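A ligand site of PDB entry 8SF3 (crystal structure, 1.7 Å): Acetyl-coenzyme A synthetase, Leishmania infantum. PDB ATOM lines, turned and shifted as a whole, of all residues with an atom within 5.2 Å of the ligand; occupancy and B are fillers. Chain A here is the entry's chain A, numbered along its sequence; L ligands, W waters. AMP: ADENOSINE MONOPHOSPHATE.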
ATOM      1  N   THR A 324      15.244 -22.942  13.443  1.00  0.00           N
ATOM      2  CA  THR A 324      14.917 -21.790  12.613  1.00  0.00           C
ATOM      3  C   THR A 324      15.411 -20.517  13.299  1.00  0.00           C
ATOM      4  O   THR A 324      15.203 -20.338  14.511  1.00  0.00           O
ATOM      5  CB  THR A 324      13.405 -21.760  12.395  1.00  0.00           C
ATOM      6  OG1 THR A 324      12.979 -23.018  11.840  1.00  0.00           O
ATOM      7  CG2 THR A 324      13.005 -20.620  11.456  1.00  0.00           C
ATOM      8  N   ILE A 370      12.290 -26.254   5.500  1.00  0.00           N
ATOM      9  CA  ILE A 370      10.915 -26.752   5.548  1.00  0.00           C
ATOM     10  C   ILE A 370      10.399 -27.113   4.162  1.00  0.00           C
ATOM     11  O   ILE A 370       9.603 -28.066   4.014  1.00  0.00           O
ATOM     12  CB  ILE A 370      10.018 -25.716   6.278  1.00  0.00           C
ATOM     13  CG1 ILE A 370       8.658 -26.338   6.594  1.00  0.00           C
ATOM     14  CG2 ILE A 370       9.853 -24.411   5.430  1.00  0.00           C
ATOM     15  CD1 ILE A 370       8.699 -27.441   7.703  1.00  0.00           C
ATOM     16  N   SER A 445       7.001 -20.894  -6.981  1.00  0.00           N
ATOM     17  CA  SER A 445       8.059 -20.077  -6.414  1.00  0.00           C
ATOM     18  C   SER A 445       7.823 -19.949  -4.921  1.00  0.00           C
ATOM     19  O   SER A 445       6.674 -19.784  -4.485  1.00  0.00           O
ATOM     20  CB  SER A 445       8.061 -18.709  -7.092  1.00  0.00           C
ATOM     21  OG  SER A 445       9.001 -17.847  -6.536  1.00  0.00           O
ATOM     22  N   VAL A 446       8.899 -20.070  -4.135  1.00  0.00           N
ATOM     23  CA  VAL A 446       8.790 -20.078  -2.682  1.00  0.00           C
ATOM     24  C   VAL A 446      10.017 -19.426  -2.075  1.00  0.00           C
ATOM     25  O   VAL A 446      11.131 -19.538  -2.590  1.00  0.00           O
ATOM     26  CB  VAL A 446       8.623 -21.516  -2.154  1.00  0.00           C
ATOM     27  CG1 VAL A 446       9.771 -22.390  -2.595  1.00  0.00           C
ATOM     28  CG2 VAL A 446       8.523 -21.507  -0.636  1.00  0.00           C
ATOM     29  N   GLY A 447       9.791 -18.761  -0.948  1.00  0.00           N
ATOM     30  CA  GLY A 447      10.829 -18.453   0.027  1.00  0.00           C
ATOM     31  C   GLY A 447      11.061 -16.974   0.253  1.00  0.00           C
ATOM     32  O   GLY A 447      11.637 -16.600   1.295  1.00  0.00           O
ATOM     33  N   GLU A 448      10.641 -16.129  -0.678  1.00  0.00           N
ATOM     34  CA  GLU A 448      10.937 -14.703  -0.684  1.00  0.00           C
ATOM     35  C   GLU A 448      10.061 -14.071  -1.765  1.00  0.00           C
ATOM     36  O   GLU A 448       9.523 -14.783  -2.613  1.00  0.00           O
ATOM     37  CB  GLU A 448      12.425 -14.442  -0.986  1.00  0.00           C
ATOM     38  CG  GLU A 448      12.869 -15.212  -2.219  1.00  0.00           C
ATOM     39  CD  GLU A 448      14.344 -15.049  -2.566  1.00  0.00           C
ATOM     40  OE1 GLU A 448      14.841 -13.904  -2.491  1.00  0.00           O
ATOM     41  OE2 GLU A 448      14.972 -16.084  -2.925  1.00  0.00           O
ATOM     42  N   PRO A 449       9.917 -12.757  -1.763  1.00  0.00           N
ATOM     43  CA  PRO A 449       9.150 -12.106  -2.831  1.00  0.00           C
ATOM     44  C   PRO A 449       9.776 -12.385  -4.197  1.00  0.00           C
ATOM     45  O   PRO A 449      10.985 -12.536  -4.320  1.00  0.00           O
ATOM     46  CB  PRO A 449       9.226 -10.626  -2.478  1.00  0.00           C
ATOM     47  CG  PRO A 449       9.571 -10.615  -0.963  1.00  0.00           C
ATOM     48  CD  PRO A 449      10.428 -11.782  -0.770  1.00  0.00           C
ATOM     49  N   ASP A 471       3.038 -18.762  -6.856  1.00  0.00           N
ATOM     50  CA  ASP A 471       3.822 -18.043  -5.841  1.00  0.00           C
ATOM     51  C   ASP A 471       3.218 -18.369  -4.477  1.00  0.00           C
ATOM     52  O   ASP A 471       2.177 -17.838  -4.108  1.00  0.00           O
ATOM     53  CB  ASP A 471       3.823 -16.548  -6.149  1.00  0.00           C
ATOM     54  CG  ASP A 471       4.568 -15.726  -5.128  1.00  0.00           C
ATOM     55  OD1 ASP A 471       5.279 -16.334  -4.315  1.00  0.00           O
ATOM     56  OD2 ASP A 471       4.455 -14.469  -5.147  1.00  0.00           O
ATOM     57  N   THR A 472       3.843 -19.278  -3.723  1.00  0.00           N
ATOM     58  CA  THR A 472       3.280 -19.786  -2.474  1.00  0.00           C
ATOM     59  C   THR A 472       3.918 -19.032  -1.310  1.00  0.00           C
ATOM     60  O   THR A 472       5.107 -19.218  -1.044  1.00  0.00           O
ATOM     61  CB  THR A 472       3.555 -21.274  -2.311  1.00  0.00           C
ATOM     62  OG1 THR A 472       4.972 -21.482  -2.312  1.00  0.00           O
ATOM     63  CG2 THR A 472       2.920 -22.122  -3.427  1.00  0.00           C
ATOM     64  N   TRP A 473       3.123 -18.254  -0.565  1.00  0.00           N
ATOM     65  CA  TRP A 473       3.592 -17.666   0.682  1.00  0.00           C
ATOM     66  C   TRP A 473       3.278 -18.625   1.820  1.00  0.00           C
ATOM     67  O   TRP A 473       2.153 -19.113   1.935  1.00  0.00           O
ATOM     68  CB  TRP A 473       2.941 -16.290   0.982  1.00  0.00           C
ATOM     69  CG  TRP A 473       3.401 -15.865   2.324  1.00  0.00           C
ATOM     70  CD1 TRP A 473       4.577 -15.255   2.603  1.00  0.00           C
ATOM     71  CD2 TRP A 473       2.781 -16.143   3.582  1.00  0.00           C
ATOM     72  NE1 TRP A 473       4.702 -15.083   3.949  1.00  0.00           N
ATOM     73  CE2 TRP A 473       3.630 -15.648   4.574  1.00  0.00           C
ATOM     74  CE3 TRP A 473       1.560 -16.724   3.968  1.00  0.00           C
ATOM     75  CZ2 TRP A 473       3.321 -15.733   5.933  1.00  0.00           C
ATOM     76  CZ3 TRP A 473       1.281 -16.814   5.307  1.00  0.00           C
ATOM     77  CH2 TRP A 473       2.148 -16.324   6.271  1.00  0.00           C
ATOM     78  N   TRP A 474       4.272 -18.876   2.671  1.00  0.00           N
ATOM     79  CA  TRP A 474       4.159 -19.625   3.914  1.00  0.00           C
ATOM     80  C   TRP A 474       5.491 -19.482   4.651  1.00  0.00           C
ATOM     81  O   TRP A 474       6.366 -18.716   4.240  1.00  0.00           O
ATOM     82  CB  TRP A 474       3.752 -21.083   3.646  1.00  0.00           C
ATOM     83  CG  TRP A 474       4.699 -21.874   2.795  1.00  0.00           C
ATOM     84  CD1 TRP A 474       5.085 -21.610   1.485  1.00  0.00           C
ATOM     85  CD2 TRP A 474       5.405 -23.052   3.187  1.00  0.00           C
ATOM     86  NE1 TRP A 474       5.960 -22.587   1.066  1.00  0.00           N
ATOM     87  CE2 TRP A 474       6.181 -23.472   2.087  1.00  0.00           C
ATOM     88  CE3 TRP A 474       5.454 -23.798   4.358  1.00  0.00           C
ATOM     89  CZ2 TRP A 474       7.006 -24.603   2.144  1.00  0.00           C
ATOM     90  CZ3 TRP A 474       6.237 -24.906   4.415  1.00  0.00           C
ATOM     91  CH2 TRP A 474       7.009 -25.303   3.308  1.00  0.00           C
ATOM     92  N   GLN A 475       5.652 -20.207   5.764  1.00  0.00           N
ATOM     93  CA  GLN A 475       6.885 -20.136   6.539  1.00  0.00           C
ATOM     94  C   GLN A 475       7.034 -21.462   7.294  1.00  0.00           C
ATOM     95  O   GLN A 475       6.096 -22.270   7.383  1.00  0.00           O
ATOM     96  CB  GLN A 475       6.868 -18.927   7.478  1.00  0.00           C
ATOM     97  CG  GLN A 475       5.565 -18.792   8.184  1.00  0.00           C
ATOM     98  CD  GLN A 475       5.354 -17.550   9.031  1.00  0.00           C
ATOM     99  OE1 GLN A 475       4.485 -17.561   9.887  1.00  0.00           O
ATOM    100  NE2 GLN A 475       6.096 -16.477   8.761  1.00  0.00           N
ATOM    101  N   THR A 476       8.236 -21.671   7.872  1.00  0.00           N
ATOM    102  CA  THR A 476       8.499 -22.914   8.605  1.00  0.00           C
ATOM    103  C   THR A 476       7.380 -23.237   9.594  1.00  0.00           C
ATOM    104  O   THR A 476       6.956 -24.395   9.705  1.00  0.00           O
ATOM    105  CB  THR A 476       9.839 -22.782   9.342  1.00  0.00           C
ATOM    106  OG1 THR A 476      10.881 -22.559   8.384  1.00  0.00           O
ATOM    107  CG2 THR A 476      10.142 -24.031  10.106  1.00  0.00           C
ATOM    108  N   GLU A 477       6.900 -22.229  10.312  1.00  0.00           N
ATOM    109  CA  GLU A 477       5.895 -22.406  11.358  1.00  0.00           C
ATOM    110  C   GLU A 477       4.534 -22.831  10.841  1.00  0.00           C
ATOM    111  O   GLU A 477       3.702 -23.245  11.642  1.00  0.00           O
ATOM    112  CB  GLU A 477       5.707 -21.105  12.129  1.00  0.00           C
ATOM    113  CG  GLU A 477       6.957 -20.610  12.819  1.00  0.00           C
ATOM    114  CD  GLU A 477       7.769 -19.607  11.992  1.00  0.00           C
ATOM    115  OE1 GLU A 477       7.731 -19.652  10.758  1.00  0.00           O
ATOM    116  OE2 GLU A 477       8.469 -18.780  12.608  1.00  0.00           O
ATOM    117  N   THR A 558       2.389 -13.539  11.855  1.00  0.00           N
ATOM    118  CA  THR A 558       3.344 -14.184  10.950  1.00  0.00           C
ATOM    119  C   THR A 558       4.745 -13.596  11.032  1.00  0.00           C
ATOM    120  O   THR A 558       5.712 -14.279  10.665  1.00  0.00           O
ATOM    121  CB  THR A 558       2.872 -14.094   9.502  1.00  0.00           C
ATOM    122  OG1 THR A 558       2.883 -12.707   9.101  1.00  0.00           O
ATOM    123  CG2 THR A 558       1.479 -14.703   9.328  1.00  0.00           C
ATOM    124  N   ASP A 560       5.398 -11.140   9.055  1.00  0.00           N
ATOM    125  CA  ASP A 560       5.425 -10.489   7.764  1.00  0.00           C
ATOM    126  C   ASP A 560       4.457  -9.315   7.694  1.00  0.00           C
ATOM    127  O   ASP A 560       3.457  -9.239   8.411  1.00  0.00           O
ATOM    128  CB  ASP A 560       5.070 -11.465   6.643  1.00  0.00           C
ATOM    129  CG  ASP A 560       6.186 -12.423   6.334  1.00  0.00           C
ATOM    130  OD1 ASP A 560       7.344 -11.963   6.206  1.00  0.00           O
ATOM    131  OD2 ASP A 560       5.907 -13.627   6.217  1.00  0.00           O
ATOM    132  N   ILE A 572       2.871  -9.838  -0.216  1.00  0.00           N
ATOM    133  CA  ILE A 572       3.697  -9.936   0.977  1.00  0.00           C
ATOM    134  C   ILE A 572       4.909  -9.035   0.774  1.00  0.00           C
ATOM    135  O   ILE A 572       5.682  -9.209  -0.167  1.00  0.00           O
ATOM    136  CB  ILE A 572       4.083 -11.384   1.281  1.00  0.00           C
ATOM    137  CG1 ILE A 572       2.908 -12.148   1.941  1.00  0.00           C
ATOM    138  CG2 ILE A 572       5.184 -11.405   2.331  1.00  0.00           C
ATOM    139  CD1 ILE A 572       1.912 -12.670   1.035  1.00  0.00           C
ATOM    140  N   GLY A 574       7.399  -8.355   3.125  1.00  0.00           N
ATOM    141  CA  GLY A 574       8.596  -8.802   3.790  1.00  0.00           C
ATOM    142  C   GLY A 574       8.451  -8.817   5.299  1.00  0.00           C
ATOM    143  O   GLY A 574       7.448  -8.386   5.859  1.00  0.00           O
ATOM    144  N   ARG A 575       9.518  -9.289   5.958  1.00  0.00           N
ATOM    145  CA  ARG A 575       9.545  -9.381   7.409  1.00  0.00           C
ATOM    146  C   ARG A 575       9.382  -8.019   8.048  1.00  0.00           C
ATOM    147  O   ARG A 575      10.002  -7.037   7.601  1.00  0.00           O
ATOM    148  CB  ARG A 575      10.875  -9.996   7.893  1.00  0.00           C
ATOM    149  CG  ARG A 575      11.165 -11.421   7.371  1.00  0.00           C
ATOM    150  CD  ARG A 575      10.184 -12.456   7.872  1.00  0.00           C
ATOM    151  NE  ARG A 575      10.150 -12.618   9.326  1.00  0.00           N
ATOM    152  CZ  ARG A 575       9.569 -13.631   9.937  1.00  0.00           C
ATOM    153  NH1 ARG A 575       9.017 -14.622   9.246  1.00  0.00           N
ATOM    154  NH2 ARG A 575       9.509 -13.647  11.272  1.00  0.00           N
ATOM    155  N   ASN A 581      16.238 -12.446   5.668  1.00  0.00           N
ATOM    156  CA  ASN A 581      15.735 -13.527   4.822  1.00  0.00           C
ATOM    157  C   ASN A 581      16.672 -13.532   3.622  1.00  0.00           C
ATOM    158  O   ASN A 581      16.476 -12.787   2.657  1.00  0.00           O
ATOM    159  CB  ASN A 581      14.236 -13.332   4.437  1.00  0.00           C
ATOM    160  CG  ASN A 581      13.609 -14.562   3.775  1.00  0.00           C
ATOM    161  OD1 ASN A 581      13.756 -15.710   4.229  1.00  0.00           O
ATOM    162  ND2 ASN A 581      12.904 -14.314   2.667  1.00  0.00           N
ATOM    163  N   GLY A 584      16.257 -16.715   0.706  1.00  0.00           N
ATOM    164  CA  GLY A 584      15.036 -17.429   1.054  1.00  0.00           C
ATOM    165  C   GLY A 584      15.039 -18.108   2.402  1.00  0.00           C
ATOM    166  O   GLY A 584      14.065 -18.800   2.718  1.00  0.00           O
ATOM    167  N   HIS A 585      16.085 -17.919   3.220  1.00  0.00           N
ATOM    168  CA  HIS A 585      16.175 -18.545   4.537  1.00  0.00           C
ATOM    169  C   HIS A 585      16.527 -17.528   5.609  1.00  0.00           C
ATOM    170  O   HIS A 585      17.379 -16.662   5.404  1.00  0.00           O
ATOM    171  CB  HIS A 585      17.202 -19.660   4.540  1.00  0.00           C
ATOM    172  CG  HIS A 585      16.932 -20.687   3.485  1.00  0.00           C
ATOM    173  ND1 HIS A 585      17.824 -21.003   2.491  1.00  0.00           N
ATOM    174  CD2 HIS A 585      15.833 -21.441   3.271  1.00  0.00           C
ATOM    175  CE1 HIS A 585      17.279 -21.912   1.696  1.00  0.00           C
ATOM    176  NE2 HIS A 585      16.072 -22.193   2.136  1.00  0.00           N
ATOM    177  N   ARG A 586      15.885 -17.684   6.755  1.00  0.00           N
ATOM    178  CA  ARG A 586      16.077 -16.740   7.840  1.00  0.00           C
ATOM    179  C   ARG A 586      17.443 -16.941   8.488  1.00  0.00           C
ATOM    180  O   ARG A 586      17.912 -18.050   8.645  1.00  0.00           O
ATOM    181  CB  ARG A 586      14.986 -16.919   8.889  1.00  0.00           C
ATOM    182  CG  ARG A 586      13.801 -16.011   8.636  1.00  0.00           C
ATOM    183  CD  ARG A 586      12.775 -16.230   9.715  1.00  0.00           C
ATOM    184  NE  ARG A 586      12.055 -17.487   9.530  1.00  0.00           N
ATOM    185  CZ  ARG A 586      11.001 -17.828  10.245  1.00  0.00           C
ATOM    186  NH1 ARG A 586      10.662 -17.175  11.353  1.00  0.00           N
ATOM    187  NH2 ARG A 586      10.237 -18.839   9.835  1.00  0.00           N
HETATM  188  P   AMP L   1      11.695 -19.385   6.539  1.00  0.00           P
HETATM  189  O1P AMP L   1      12.878 -19.016   7.429  1.00  0.00           O
HETATM  190  O2P AMP L   1      12.152 -20.068   5.272  1.00  0.00           O
HETATM  191  O3P AMP L   1      10.586 -20.029   7.331  1.00  0.00           O
HETATM  192  O5' AMP L   1      11.188 -17.976   6.017  1.00  0.00           O
HETATM  193  C5' AMP L   1       9.811 -17.670   5.979  1.00  0.00           C
HETATM  194  C4' AMP L   1       9.668 -16.283   5.451  1.00  0.00           C
HETATM  195  O4' AMP L   1      10.069 -16.272   4.067  1.00  0.00           O
HETATM  196  C3' AMP L   1       8.290 -15.688   5.440  1.00  0.00           C
HETATM  197  O3' AMP L   1       7.894 -15.242   6.733  1.00  0.00           O
HETATM  198  C2' AMP L   1       8.430 -14.584   4.402  1.00  0.00           C
HETATM  199  O2' AMP L   1       9.081 -13.443   4.922  1.00  0.00           O
HETATM  200  C1' AMP L   1       9.358 -15.251   3.382  1.00  0.00           C
HETATM  201  N9  AMP L   1       8.596 -15.858   2.293  1.00  0.00           N
HETATM  202  C8  AMP L   1       8.393 -17.175   2.085  1.00  0.00           C
HETATM  203  N7  AMP L   1       7.659 -17.377   0.947  1.00  0.00           N
HETATM  204  C5  AMP L   1       7.394 -16.149   0.454  1.00  0.00           C
HETATM  205  C6  AMP L   1       6.687 -15.622  -0.720  1.00  0.00           C
HETATM  206  N6  AMP L   1       6.110 -16.468  -1.558  1.00  0.00           N
HETATM  207  N1  AMP L   1       6.636 -14.304  -0.891  1.00  0.00           N
HETATM  208  C2  AMP L   1       7.232 -13.453  -0.031  1.00  0.00           C
HETATM  209  N3  AMP L   1       7.913 -13.852   1.052  1.00  0.00           N
HETATM  210  C4  AMP L   1       8.029 -15.165   1.318  1.00  0.00           C
HETATM  211  O   HOH W   1      14.703 -21.001   8.137  1.00  0.00           O
HETATM  212  O   HOH W   2       8.079 -16.529  -4.344  1.00  0.00           O
HETATM  213  O   HOH W   3      13.538 -22.204   4.905  1.00  0.00           O
HETATM  214  O   HOH W   4      12.000 -17.854   3.547  1.00  0.00           O
HETATM  215  O   HOH W   5       9.253 -11.948   2.576  1.00  0.00           O
HETATM  216  O   HOH W   6       4.252 -13.942  -2.563  1.00  0.00           O
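Water W6 bridges OD2 of Asp 471 and N1 of the ligand. Water W2 lies within hydrogen-bond range of OG of Ser 445, OD1 of Asp 471, O of Glu 448 and N6 of the ligand.
The backbone carbonyl oxygen of Glu 448 sits close to a nitrogen (N1) of the ligand. O of Gly 584 lies close to O2P of the ligand, 3.4 Å away. N of Pro 449 touches C2 of the ligand, at 3.3 Å. Trp 473 touches the ligand. Trp 474 touches the ligand (O to C8, 3.3 Å). CG2 of Ile 572 touches C2 of the ligand (3.7 Å). ND2 of Asn 581 touches O4' of the ligand, 3.7 Å away. 15 residues have an atom within 4 Å of the ligand: Gly 447, Glu 448, Pro 449, Asp 471, Thr 472, Trp 473, Trp 474, Gln 475, Thr 476, Asp 560, Ile 572, Arg 575, Asn 581, Gly 584 and Arg 586.
An oxygen (O1P) of the ligand is in salt-bridge range of the guanidinium group (NE) of Arg 586 (2.7 Å). The backbone NH (N) of Gly 447 sits at hydrogen-bond distance from a nitrogen (N7) of the ligand. O of Thr 472 is in hydrogen-bond range of N6 of the ligand (3.0 Å). OG1 of Thr 476 lies within hydrogen-bond range of O3P of the ligand (2.8 Å). An oxygen (O3P) of the ligand lies within hydrogen-bond range of the backbone NH (N) of Thr 476 (2.9 Å). An oxygen (O3') of the ligand is in hydrogen-bond range of the guanidinium group (NH1) of Arg 575 (2.8 Å). OD1 of Asp 471 lies within hydrogen-bond range of N6 of the ligand, 2.9 Å away. OD2 of Asp 560 sits at hydrogen-bond distance from O3' of the ligand (2.6 Å). NE2 of Gln 475 lies within hydrogen-bond range of O3' of the ligand (3.0 Å). An oxygen (O1P) of the ligand sits close to the backbone NH of Arg 586 (3.4 Å).
N of Thr 472 lies within hydrogen-bond range of O of Ser 445, at 3.0 Å. The backbone NH (N) of Asp 560 sits at hydrogen-bond distance from the side-chain hydroxyl (OG1) of Thr 558 (3.0 Å). OD1 of Asn 581 lies close to O of Gly 584, at 3.5 Å. The backbone carbonyl oxygen (O) of Gly 447 sits at hydrogen-bond distance from the side-chain amide nitrogen (ND2) of Asn 581 (3.0 Å). OE1 of Glu 477 lies within salt-bridge range of NH2 of Arg 586, at 2.8 Å. The side-chain carboxylate (OD2) of Asp 560 is in hydrogen-bond range of the indole nitrogen (NE1) of Trp 473, at 3.0 Å. NH1 of Arg 575 lies close to NE2 of Gln 475 (3.5 Å). OD1 of Asn 581 lies within hydrogen-bond range of N of His 585, 3.4 Å away.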
